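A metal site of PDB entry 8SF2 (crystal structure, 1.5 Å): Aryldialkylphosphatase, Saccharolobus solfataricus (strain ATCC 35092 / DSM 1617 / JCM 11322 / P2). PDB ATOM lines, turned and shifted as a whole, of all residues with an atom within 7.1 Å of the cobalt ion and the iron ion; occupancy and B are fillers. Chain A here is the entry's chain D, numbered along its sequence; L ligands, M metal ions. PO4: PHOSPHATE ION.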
ATOM      1  N   HIS A  22      -9.041   1.774  34.027  1.00  0.00           N
ATOM      2  CA  HIS A  22      -8.401   1.822  32.716  1.00  0.00           C
ATOM      3  C   HIS A  22      -7.221   0.845  32.671  1.00  0.00           C
ATOM      4  O   HIS A  22      -6.082   1.215  32.970  1.00  0.00           O
ATOM      5  CB  HIS A  22      -7.975   3.242  32.359  1.00  0.00           C
ATOM      6  CG  HIS A  22      -7.555   3.422  30.926  1.00  0.00           C
ATOM      7  ND1 HIS A  22      -7.940   4.517  30.188  1.00  0.00           N
ATOM      8  CD2 HIS A  22      -6.772   2.684  30.120  1.00  0.00           C
ATOM      9  CE1 HIS A  22      -7.422   4.427  28.971  1.00  0.00           C
ATOM     10  NE2 HIS A  22      -6.706   3.322  28.900  1.00  0.00           N
ATOM     11  N   GLU A  23      -7.504  -0.402  32.279  1.00  0.00           N
ATOM     12  CA  GLU A  23      -6.499  -1.425  32.081  1.00  0.00           C
ATOM     13  C   GLU A  23      -6.849  -2.212  30.815  1.00  0.00           C
ATOM     14  O   GLU A  23      -8.010  -2.255  30.407  1.00  0.00           O
ATOM     15  CB  GLU A  23      -6.446  -2.413  33.257  1.00  0.00           C
ATOM     16  CG  GLU A  23      -6.377  -1.736  34.621  1.00  0.00           C
ATOM     17  CD  GLU A  23      -5.082  -1.001  34.915  1.00  0.00           C
ATOM     18  OE1 GLU A  23      -5.093  -0.134  35.805  1.00  0.00           O
ATOM     19  OE2 GLU A  23      -4.069  -1.289  34.248  1.00  0.00           O
ATOM     20  N   HIS A  24      -5.845  -2.826  30.205  1.00  0.00           N
ATOM     21  CA  HIS A  24      -6.038  -3.581  28.973  1.00  0.00           C
ATOM     22  C   HIS A  24      -5.568  -5.014  29.161  1.00  0.00           C
ATOM     23  O   HIS A  24      -4.392  -5.261  29.438  1.00  0.00           O
ATOM     24  CB  HIS A  24      -5.242  -2.962  27.824  1.00  0.00           C
ATOM     25  CG  HIS A  24      -5.640  -1.567  27.475  1.00  0.00           C
ATOM     26  ND1 HIS A  24      -6.650  -1.256  26.597  1.00  0.00           N
ATOM     27  CD2 HIS A  24      -5.109  -0.384  27.867  1.00  0.00           C
ATOM     28  CE1 HIS A  24      -6.739   0.062  26.479  1.00  0.00           C
ATOM     29  NE2 HIS A  24      -5.813   0.615  27.239  1.00  0.00           N
ATOM     30  N   PRO A  67     -10.853  -0.469  28.308  1.00  0.00           N
ATOM     31  CA  PRO A  67     -11.268   0.347  27.160  1.00  0.00           C
ATOM     32  C   PRO A  67     -10.578  -0.001  25.846  1.00  0.00           C
ATOM     33  O   PRO A  67     -10.305   0.873  25.032  1.00  0.00           O
ATOM     34  CB  PRO A  67     -10.913   1.763  27.618  1.00  0.00           C
ATOM     35  CG  PRO A  67      -9.687   1.575  28.485  1.00  0.00           C
ATOM     36  CD  PRO A  67      -9.831   0.201  29.129  1.00  0.00           C
ATOM     37  N   THR A  68     -10.304  -1.291  25.642  1.00  0.00           N
ATOM     38  CA  THR A  68      -9.828  -1.772  24.349  1.00  0.00           C
ATOM     39  C   THR A  68     -11.005  -1.796  23.378  1.00  0.00           C
ATOM     40  O   THR A  68     -12.000  -2.491  23.627  1.00  0.00           O
ATOM     41  CB  THR A  68      -9.238  -3.187  24.477  1.00  0.00           C
ATOM     42  OG1 THR A  68      -8.286  -3.239  25.536  1.00  0.00           O
ATOM     43  CG2 THR A  68      -8.572  -3.630  23.186  1.00  0.00           C
ATOM     44  N   LEU A  72      -7.503  -0.991  18.779  1.00  0.00           N
ATOM     45  CA  LEU A  72      -6.660  -1.585  19.812  1.00  0.00           C
ATOM     46  C   LEU A  72      -6.877  -3.085  19.936  1.00  0.00           C
ATOM     47  O   LEU A  72      -6.273  -3.705  20.820  1.00  0.00           O
ATOM     48  CB  LEU A  72      -6.950  -0.908  21.159  1.00  0.00           C
ATOM     49  CG  LEU A  72      -6.744   0.606  21.229  1.00  0.00           C
ATOM     50  CD1 LEU A  72      -7.265   1.167  22.539  1.00  0.00           C
ATOM     51  CD2 LEU A  72      -5.270   0.957  21.056  1.00  0.00           C
ATOM     52  N   TYR A  97     -10.840   4.084  18.428  1.00  0.00           N
ATOM     53  CA  TYR A  97      -9.584   4.689  18.825  1.00  0.00           C
ATOM     54  C   TYR A  97      -8.819   5.054  17.549  1.00  0.00           C
ATOM     55  O   TYR A  97      -8.259   4.185  16.888  1.00  0.00           O
ATOM     56  CB  TYR A  97      -8.817   3.689  19.696  1.00  0.00           C
ATOM     57  CG  TYR A  97      -7.526   4.168  20.292  1.00  0.00           C
ATOM     58  CD1 TYR A  97      -6.345   4.147  19.563  1.00  0.00           C
ATOM     59  CD2 TYR A  97      -7.462   4.554  21.617  1.00  0.00           C
ATOM     60  CE1 TYR A  97      -5.148   4.542  20.121  1.00  0.00           C
ATOM     61  CE2 TYR A  97      -6.266   4.943  22.198  1.00  0.00           C
ATOM     62  CZ  TYR A  97      -5.105   4.936  21.448  1.00  0.00           C
ATOM     63  OH  TYR A  97      -3.917   5.315  22.022  1.00  0.00           O
ATOM     64  N   TYR A  99      -6.384   8.609  15.854  1.00  0.00           N
ATOM     65  CA  TYR A  99      -5.749   9.903  16.080  1.00  0.00           C
ATOM     66  C   TYR A  99      -6.004  10.859  14.921  1.00  0.00           C
ATOM     67  O   TYR A  99      -5.982  12.071  15.132  1.00  0.00           O
ATOM     68  CB  TYR A  99      -4.234   9.759  16.258  1.00  0.00           C
ATOM     69  CG  TYR A  99      -3.774   9.077  17.533  1.00  0.00           C
ATOM     70  CD1 TYR A  99      -4.666   8.613  18.485  1.00  0.00           C
ATOM     71  CD2 TYR A  99      -2.418   8.907  17.771  1.00  0.00           C
ATOM     72  CE1 TYR A  99      -4.222   7.980  19.641  1.00  0.00           C
ATOM     73  CE2 TYR A  99      -1.963   8.280  18.921  1.00  0.00           C
ATOM     74  CZ  TYR A  99      -2.868   7.807  19.858  1.00  0.00           C
ATOM     75  OH  TYR A  99      -2.394   7.183  20.996  1.00  0.00           O
ATOM     76  N   KCX A 137     -15.489   4.513  24.391  1.00  0.00           N
ATOM     77  CA  KCX A 137     -14.086   4.977  24.392  1.00  0.00           C
ATOM     78  CB  KCX A 137     -13.143   3.781  24.508  1.00  0.00           C
ATOM     79  CG  KCX A 137     -11.673   4.113  24.279  1.00  0.00           C
ATOM     80  CD  KCX A 137     -11.112   5.016  25.349  1.00  0.00           C
ATOM     81  CE  KCX A 137      -9.628   5.279  25.168  1.00  0.00           C
ATOM     82  NZ  KCX A 137      -8.837   4.059  25.377  1.00  0.00           N
ATOM     83  C   KCX A 137     -13.814   5.764  23.108  1.00  0.00           C
ATOM     84  O   KCX A 137     -14.091   5.249  22.026  1.00  0.00           O
ATOM     85  CX  KCX A 137      -7.542   4.129  25.681  1.00  0.00           C
ATOM     86  OQ1 KCX A 137      -6.954   2.973  25.839  1.00  0.00           O
ATOM     87  OQ2 KCX A 137      -6.936   5.191  25.791  1.00  0.00           O
ATOM     88  N   ILE A 138     -13.249   6.996  23.282  1.00  0.00           N
ATOM     89  CA  ILE A 138     -12.852   7.853  22.135  1.00  0.00           C
ATOM     90  C   ILE A 138     -11.427   8.333  22.404  1.00  0.00           C
ATOM     91  O   ILE A 138     -10.952   8.269  23.541  1.00  0.00           O
ATOM     92  CB  ILE A 138     -13.824   9.028  21.965  1.00  0.00           C
ATOM     93  CG1 ILE A 138     -13.784   9.944  23.188  1.00  0.00           C
ATOM     94  CG2 ILE A 138     -15.228   8.542  21.695  1.00  0.00           C
ATOM     95  CD1 ILE A 138     -14.633  11.187  23.073  1.00  0.00           C
ATOM     96  N   ALA A 139     -10.753   8.827  21.362  1.00  0.00           N
ATOM     97  CA  ALA A 139      -9.360   9.249  21.473  1.00  0.00           C
ATOM     98  C   ALA A 139      -9.092  10.515  20.658  1.00  0.00           C
ATOM     99  O   ALA A 139      -9.753  10.796  19.661  1.00  0.00           O
ATOM    100  CB  ALA A 139      -8.418   8.150  21.020  1.00  0.00           C
ATOM    101  N   ASP A 141      -5.047  12.793  20.077  1.00  0.00           N
ATOM    102  CA  ASP A 141      -3.677  12.877  20.535  1.00  0.00           C
ATOM    103  C   ASP A 141      -2.996  14.065  19.877  1.00  0.00           C
ATOM    104  O   ASP A 141      -3.612  15.127  19.734  1.00  0.00           O
ATOM    105  CB  ASP A 141      -2.949  11.542  20.311  1.00  0.00           C
ATOM    106  CG  ASP A 141      -1.791  11.326  21.266  1.00  0.00           C
ATOM    107  OD1 ASP A 141      -0.706  11.915  21.052  1.00  0.00           O
ATOM    108  OD2 ASP A 141      -1.974  10.569  22.250  1.00  0.00           O
ATOM    109  N   THR A 169     -12.160   8.794  27.712  1.00  0.00           N
ATOM    110  CA  THR A 169     -11.348   9.302  26.622  1.00  0.00           C
ATOM    111  C   THR A 169      -9.876   8.960  26.798  1.00  0.00           C
ATOM    112  O   THR A 169      -9.388   8.718  27.912  1.00  0.00           O
ATOM    113  CB  THR A 169     -11.488  10.821  26.410  1.00  0.00           C
ATOM    114  OG1 THR A 169     -10.540  11.505  27.242  1.00  0.00           O
ATOM    115  CG2 THR A 169     -12.885  11.328  26.672  1.00  0.00           C
ATOM    116  N   HIS A 170      -9.198   8.929  25.661  1.00  0.00           N
ATOM    117  CA  HIS A 170      -7.753   9.037  25.559  1.00  0.00           C
ATOM    118  C   HIS A 170      -7.456  10.457  25.093  1.00  0.00           C
ATOM    119  O   HIS A 170      -8.067  10.907  24.127  1.00  0.00           O
ATOM    120  CB  HIS A 170      -7.242   8.046  24.515  1.00  0.00           C
ATOM    121  CG  HIS A 170      -5.812   8.227  24.120  1.00  0.00           C
ATOM    122  ND1 HIS A 170      -4.853   7.324  24.514  1.00  0.00           N
ATOM    123  CD2 HIS A 170      -5.179   9.154  23.392  1.00  0.00           C
ATOM    124  CE1 HIS A 170      -3.680   7.693  24.021  1.00  0.00           C
ATOM    125  NE2 HIS A 170      -3.850   8.807  23.339  1.00  0.00           N
ATOM    126  N   SER A 171      -6.535  11.146  25.777  1.00  0.00           N
ATOM    127  CA  SER A 171      -6.113  12.469  25.337  1.00  0.00           C
ATOM    128  C   SER A 171      -4.595  12.570  25.459  1.00  0.00           C
ATOM    129  O   SER A 171      -3.943  11.708  26.053  1.00  0.00           O
ATOM    130  CB  SER A 171      -6.809  13.579  26.121  1.00  0.00           C
ATOM    131  OG  SER A 171      -6.143  13.872  27.337  1.00  0.00           O
ATOM    132  N   GLY A 198      -8.970  11.228  29.816  1.00  0.00           N
ATOM    133  CA  GLY A 198      -7.886  10.306  30.064  1.00  0.00           C
ATOM    134  C   GLY A 198      -6.507  10.940  29.954  1.00  0.00           C
ATOM    135  O   GLY A 198      -6.304  11.934  29.231  1.00  0.00           O
ATOM    136  N   HIS A 199      -5.571  10.356  30.708  1.00  0.00           N
ATOM    137  CA  HIS A 199      -4.138  10.543  30.556  1.00  0.00           C
ATOM    138  C   HIS A 199      -3.681  11.897  31.079  1.00  0.00           C
ATOM    139  O   HIS A 199      -2.580  12.347  30.760  1.00  0.00           O
ATOM    140  CB  HIS A 199      -3.693  10.261  29.123  1.00  0.00           C
ATOM    141  CG  HIS A 199      -4.104   8.909  28.631  1.00  0.00           C
ATOM    142  ND1 HIS A 199      -4.322   7.844  29.478  1.00  0.00           N
ATOM    143  CD2 HIS A 199      -4.327   8.449  27.399  1.00  0.00           C
ATOM    144  CE1 HIS A 199      -4.690   6.783  28.767  1.00  0.00           C
ATOM    145  NE2 HIS A 199      -4.695   7.128  27.502  1.00  0.00           N
ATOM    146  N   ASP A 222      -3.977   7.942  35.142  1.00  0.00           N
ATOM    147  CA  ASP A 222      -4.363   6.596  34.729  1.00  0.00           C
ATOM    148  C   ASP A 222      -3.239   5.845  34.020  1.00  0.00           C
ATOM    149  O   ASP A 222      -3.502   4.793  33.433  1.00  0.00           O
ATOM    150  CB  ASP A 222      -5.621   6.654  33.855  1.00  0.00           C
ATOM    151  CG  ASP A 222      -5.503   7.551  32.633  1.00  0.00           C
ATOM    152  OD1 ASP A 222      -4.363   7.860  32.228  1.00  0.00           O
ATOM    153  OD2 ASP A 222      -6.553   7.938  32.084  1.00  0.00           O
ATOM    154  N   ARG A 223      -1.998   6.324  34.131  1.00  0.00           N
ATOM    155  CA  ARG A 223      -0.885   5.668  33.466  1.00  0.00           C
ATOM    156  C   ARG A 223       0.280   5.430  34.427  1.00  0.00           C
ATOM    157  O   ARG A 223       1.441   5.500  34.029  1.00  0.00           O
ATOM    158  CB  ARG A 223      -0.421   6.470  32.242  1.00  0.00           C
ATOM    159  CG  ARG A 223      -1.281   6.235  31.016  1.00  0.00           C
ATOM    160  CD  ARG A 223      -0.913   7.152  29.864  1.00  0.00           C
ATOM    161  NE  ARG A 223      -1.282   6.530  28.602  1.00  0.00           N
ATOM    162  CZ  ARG A 223      -1.096   7.084  27.412  1.00  0.00           C
ATOM    163  NH1 ARG A 223      -0.606   8.313  27.304  1.00  0.00           N
ATOM    164  NH2 ARG A 223      -1.416   6.401  26.329  1.00  0.00           N
ATOM    165  N   ASP A 256      -3.228   1.808  33.006  1.00  0.00           N
ATOM    166  CA  ASP A 256      -3.248   1.694  31.554  1.00  0.00           C
ATOM    167  C   ASP A 256      -2.313   0.563  31.151  1.00  0.00           C
ATOM    168  O   ASP A 256      -1.715   0.578  30.075  1.00  0.00           O
ATOM    169  CB  ASP A 256      -2.827   3.001  30.881  1.00  0.00           C
ATOM    170  CG  ASP A 256      -3.188   3.092  29.406  1.00  0.00           C
ATOM    171  OD1 ASP A 256      -3.984   2.250  28.924  1.00  0.00           O
ATOM    172  OD2 ASP A 256      -2.689   4.027  28.737  1.00  0.00           O
ATOM    173  N   TYR A 257      -2.175  -0.410  32.053  1.00  0.00           N
ATOM    174  CA  TYR A 257      -1.247  -1.492  31.807  1.00  0.00           C
ATOM    175  C   TYR A 257      -1.824  -2.381  30.723  1.00  0.00           C
ATOM    176  O   TYR A 257      -2.997  -2.768  30.783  1.00  0.00           O
ATOM    177  CB  TYR A 257      -0.960  -2.329  33.043  1.00  0.00           C
ATOM    178  CG  TYR A 257       0.062  -3.408  32.787  1.00  0.00           C
ATOM    179  CD1 TYR A 257       1.381  -3.086  32.543  1.00  0.00           C
ATOM    180  CD2 TYR A 257      -0.297  -4.743  32.754  1.00  0.00           C
ATOM    181  CE1 TYR A 257       2.333  -4.060  32.285  1.00  0.00           C
ATOM    182  CE2 TYR A 257       0.641  -5.733  32.505  1.00  0.00           C
ATOM    183  CZ  TYR A 257       1.955  -5.385  32.276  1.00  0.00           C
ATOM    184  OH  TYR A 257       2.890  -6.372  32.040  1.00  0.00           O
ATOM    185  N   CYS A 258      -0.995  -2.697  29.735  1.00  0.00           N
ATOM    186  CA  CYS A 258      -1.347  -3.639  28.689  1.00  0.00           C
ATOM    187  C   CYS A 258      -0.600  -4.935  28.934  1.00  0.00           C
ATOM    188  O   CYS A 258       0.618  -4.988  28.791  1.00  0.00           O
ATOM    189  CB  CYS A 258      -1.002  -3.079  27.309  1.00  0.00           C
ATOM    190  SG  CYS A 258      -1.793  -1.500  26.968  1.00  0.00           S
ATOM    191  N   TRP A 263       2.780  -2.816  20.027  1.00  0.00           N
ATOM    192  CA  TRP A 263       3.489  -1.623  19.574  1.00  0.00           C
ATOM    193  C   TRP A 263       4.991  -1.814  19.760  1.00  0.00           C
ATOM    194  O   TRP A 263       5.430  -2.493  20.696  1.00  0.00           O
ATOM    195  CB  TRP A 263       3.004  -0.371  20.327  1.00  0.00           C
ATOM    196  CG  TRP A 263       1.556  -0.026  20.148  1.00  0.00           C
ATOM    197  CD1 TRP A 263       0.595  -0.779  19.522  1.00  0.00           C
ATOM    198  CD2 TRP A 263       0.888   1.169  20.601  1.00  0.00           C
ATOM    199  NE1 TRP A 263      -0.622  -0.130  19.560  1.00  0.00           N
ATOM    200  CE2 TRP A 263      -0.470   1.062  20.218  1.00  0.00           C
ATOM    201  CE3 TRP A 263       1.311   2.306  21.292  1.00  0.00           C
ATOM    202  CZ2 TRP A 263      -1.397   2.064  20.497  1.00  0.00           C
ATOM    203  CZ3 TRP A 263       0.386   3.298  21.581  1.00  0.00           C
ATOM    204  CH2 TRP A 263      -0.951   3.172  21.184  1.00  0.00           C
HETATM  205  P   PO4 L   1      -3.734   3.792  25.739  1.00  0.00           P
HETATM  206  O1  PO4 L   1      -2.234   3.780  26.046  1.00  0.00           O
HETATM  207  O2  PO4 L   1      -4.527   4.317  26.910  1.00  0.00           O
HETATM  208  O3  PO4 L   1      -4.175   2.383  25.357  1.00  0.00           O
HETATM  209  O4  PO4 L   1      -3.999   4.722  24.597  1.00  0.00           O
HETATM  210 CO    CO M   1      -5.010   5.819  25.888  1.00  0.00          CO
HETATM  211 FE    FE M   2      -5.485   2.648  27.351  1.00  0.00          FE
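OH of Tyr 97 lies close to ND1 of His 170, at 3.3 Å.
The side-chain hydroxyl (OH) of Tyr 99 sits at hydrogen-bond distance from a ring nitrogen (NE2) of His 170 (3.2 Å).
NE2 of His 170 sits at hydrogen-bond distance from OD2 of Asp 141.
A ring nitrogen (ND1) of His 199 is in hydrogen-bond range of the side-chain carboxylate (OD1) of Asp 222, at 2.8 Å.
The side-chain carboxylate of Asp 256 is in salt-bridge range of the guanidinium group of Arg 223.
The backbone carbonyl oxygen (O) of Asp 256 lies within hydrogen-bond range of the side-chain sulfur (SG) of Cys 258 (3.7 Å).
N of Asp 256 is in hydrogen-bond range of O of Asp 222, 3.0 Å away.
The side-chain hydroxyl (OH) of Tyr 99 is in hydrogen-bond range of the side-chain hydroxyl (OH) of Tyr 97 (2.6 Å).
Merely in contact with the cobalt ion: Arg 223 (3.7 Å) and Tyr 97 (3.995 Å).
The nearest printed residue that does not touch the cobalt ion is Asp 256 (4.1 Å).
Four residues have an atom within 4 Å of the iron ion: His 22, His 24, KCX 137 and Asp 256.
The nearest printed residue that does not touch the iron ion is His 199 (4.4 Å).
The cobalt ion is bound by an oxygen (O2) of the ligand (1.9 Å), an oxygen (O4) of the ligand (2.0 Å), OQ2 of KCX 137 (2.0 Å), a ring nitrogen (ND1) of His 170 (2.0 Å) and a ring nitrogen (NE2) of His 199 (2.1 Å).
O2 of the ligand binds the iron ion.
The iron ion is bound by NE2 of His 24 (2.1 Å).
The iron ion is bound by a ring nitrogen (NE2) of His 22 (2.1 Å).
The iron ion is bound by OQ1 of KCX 137, 2.1 Å away.
OD1 of Asp 256 is bound to the iron ion, 2.2 Å away.
The iron ion is bound by O3 of the ligand (2.4 Å).
The iron ion has six donor atoms within binding distance.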
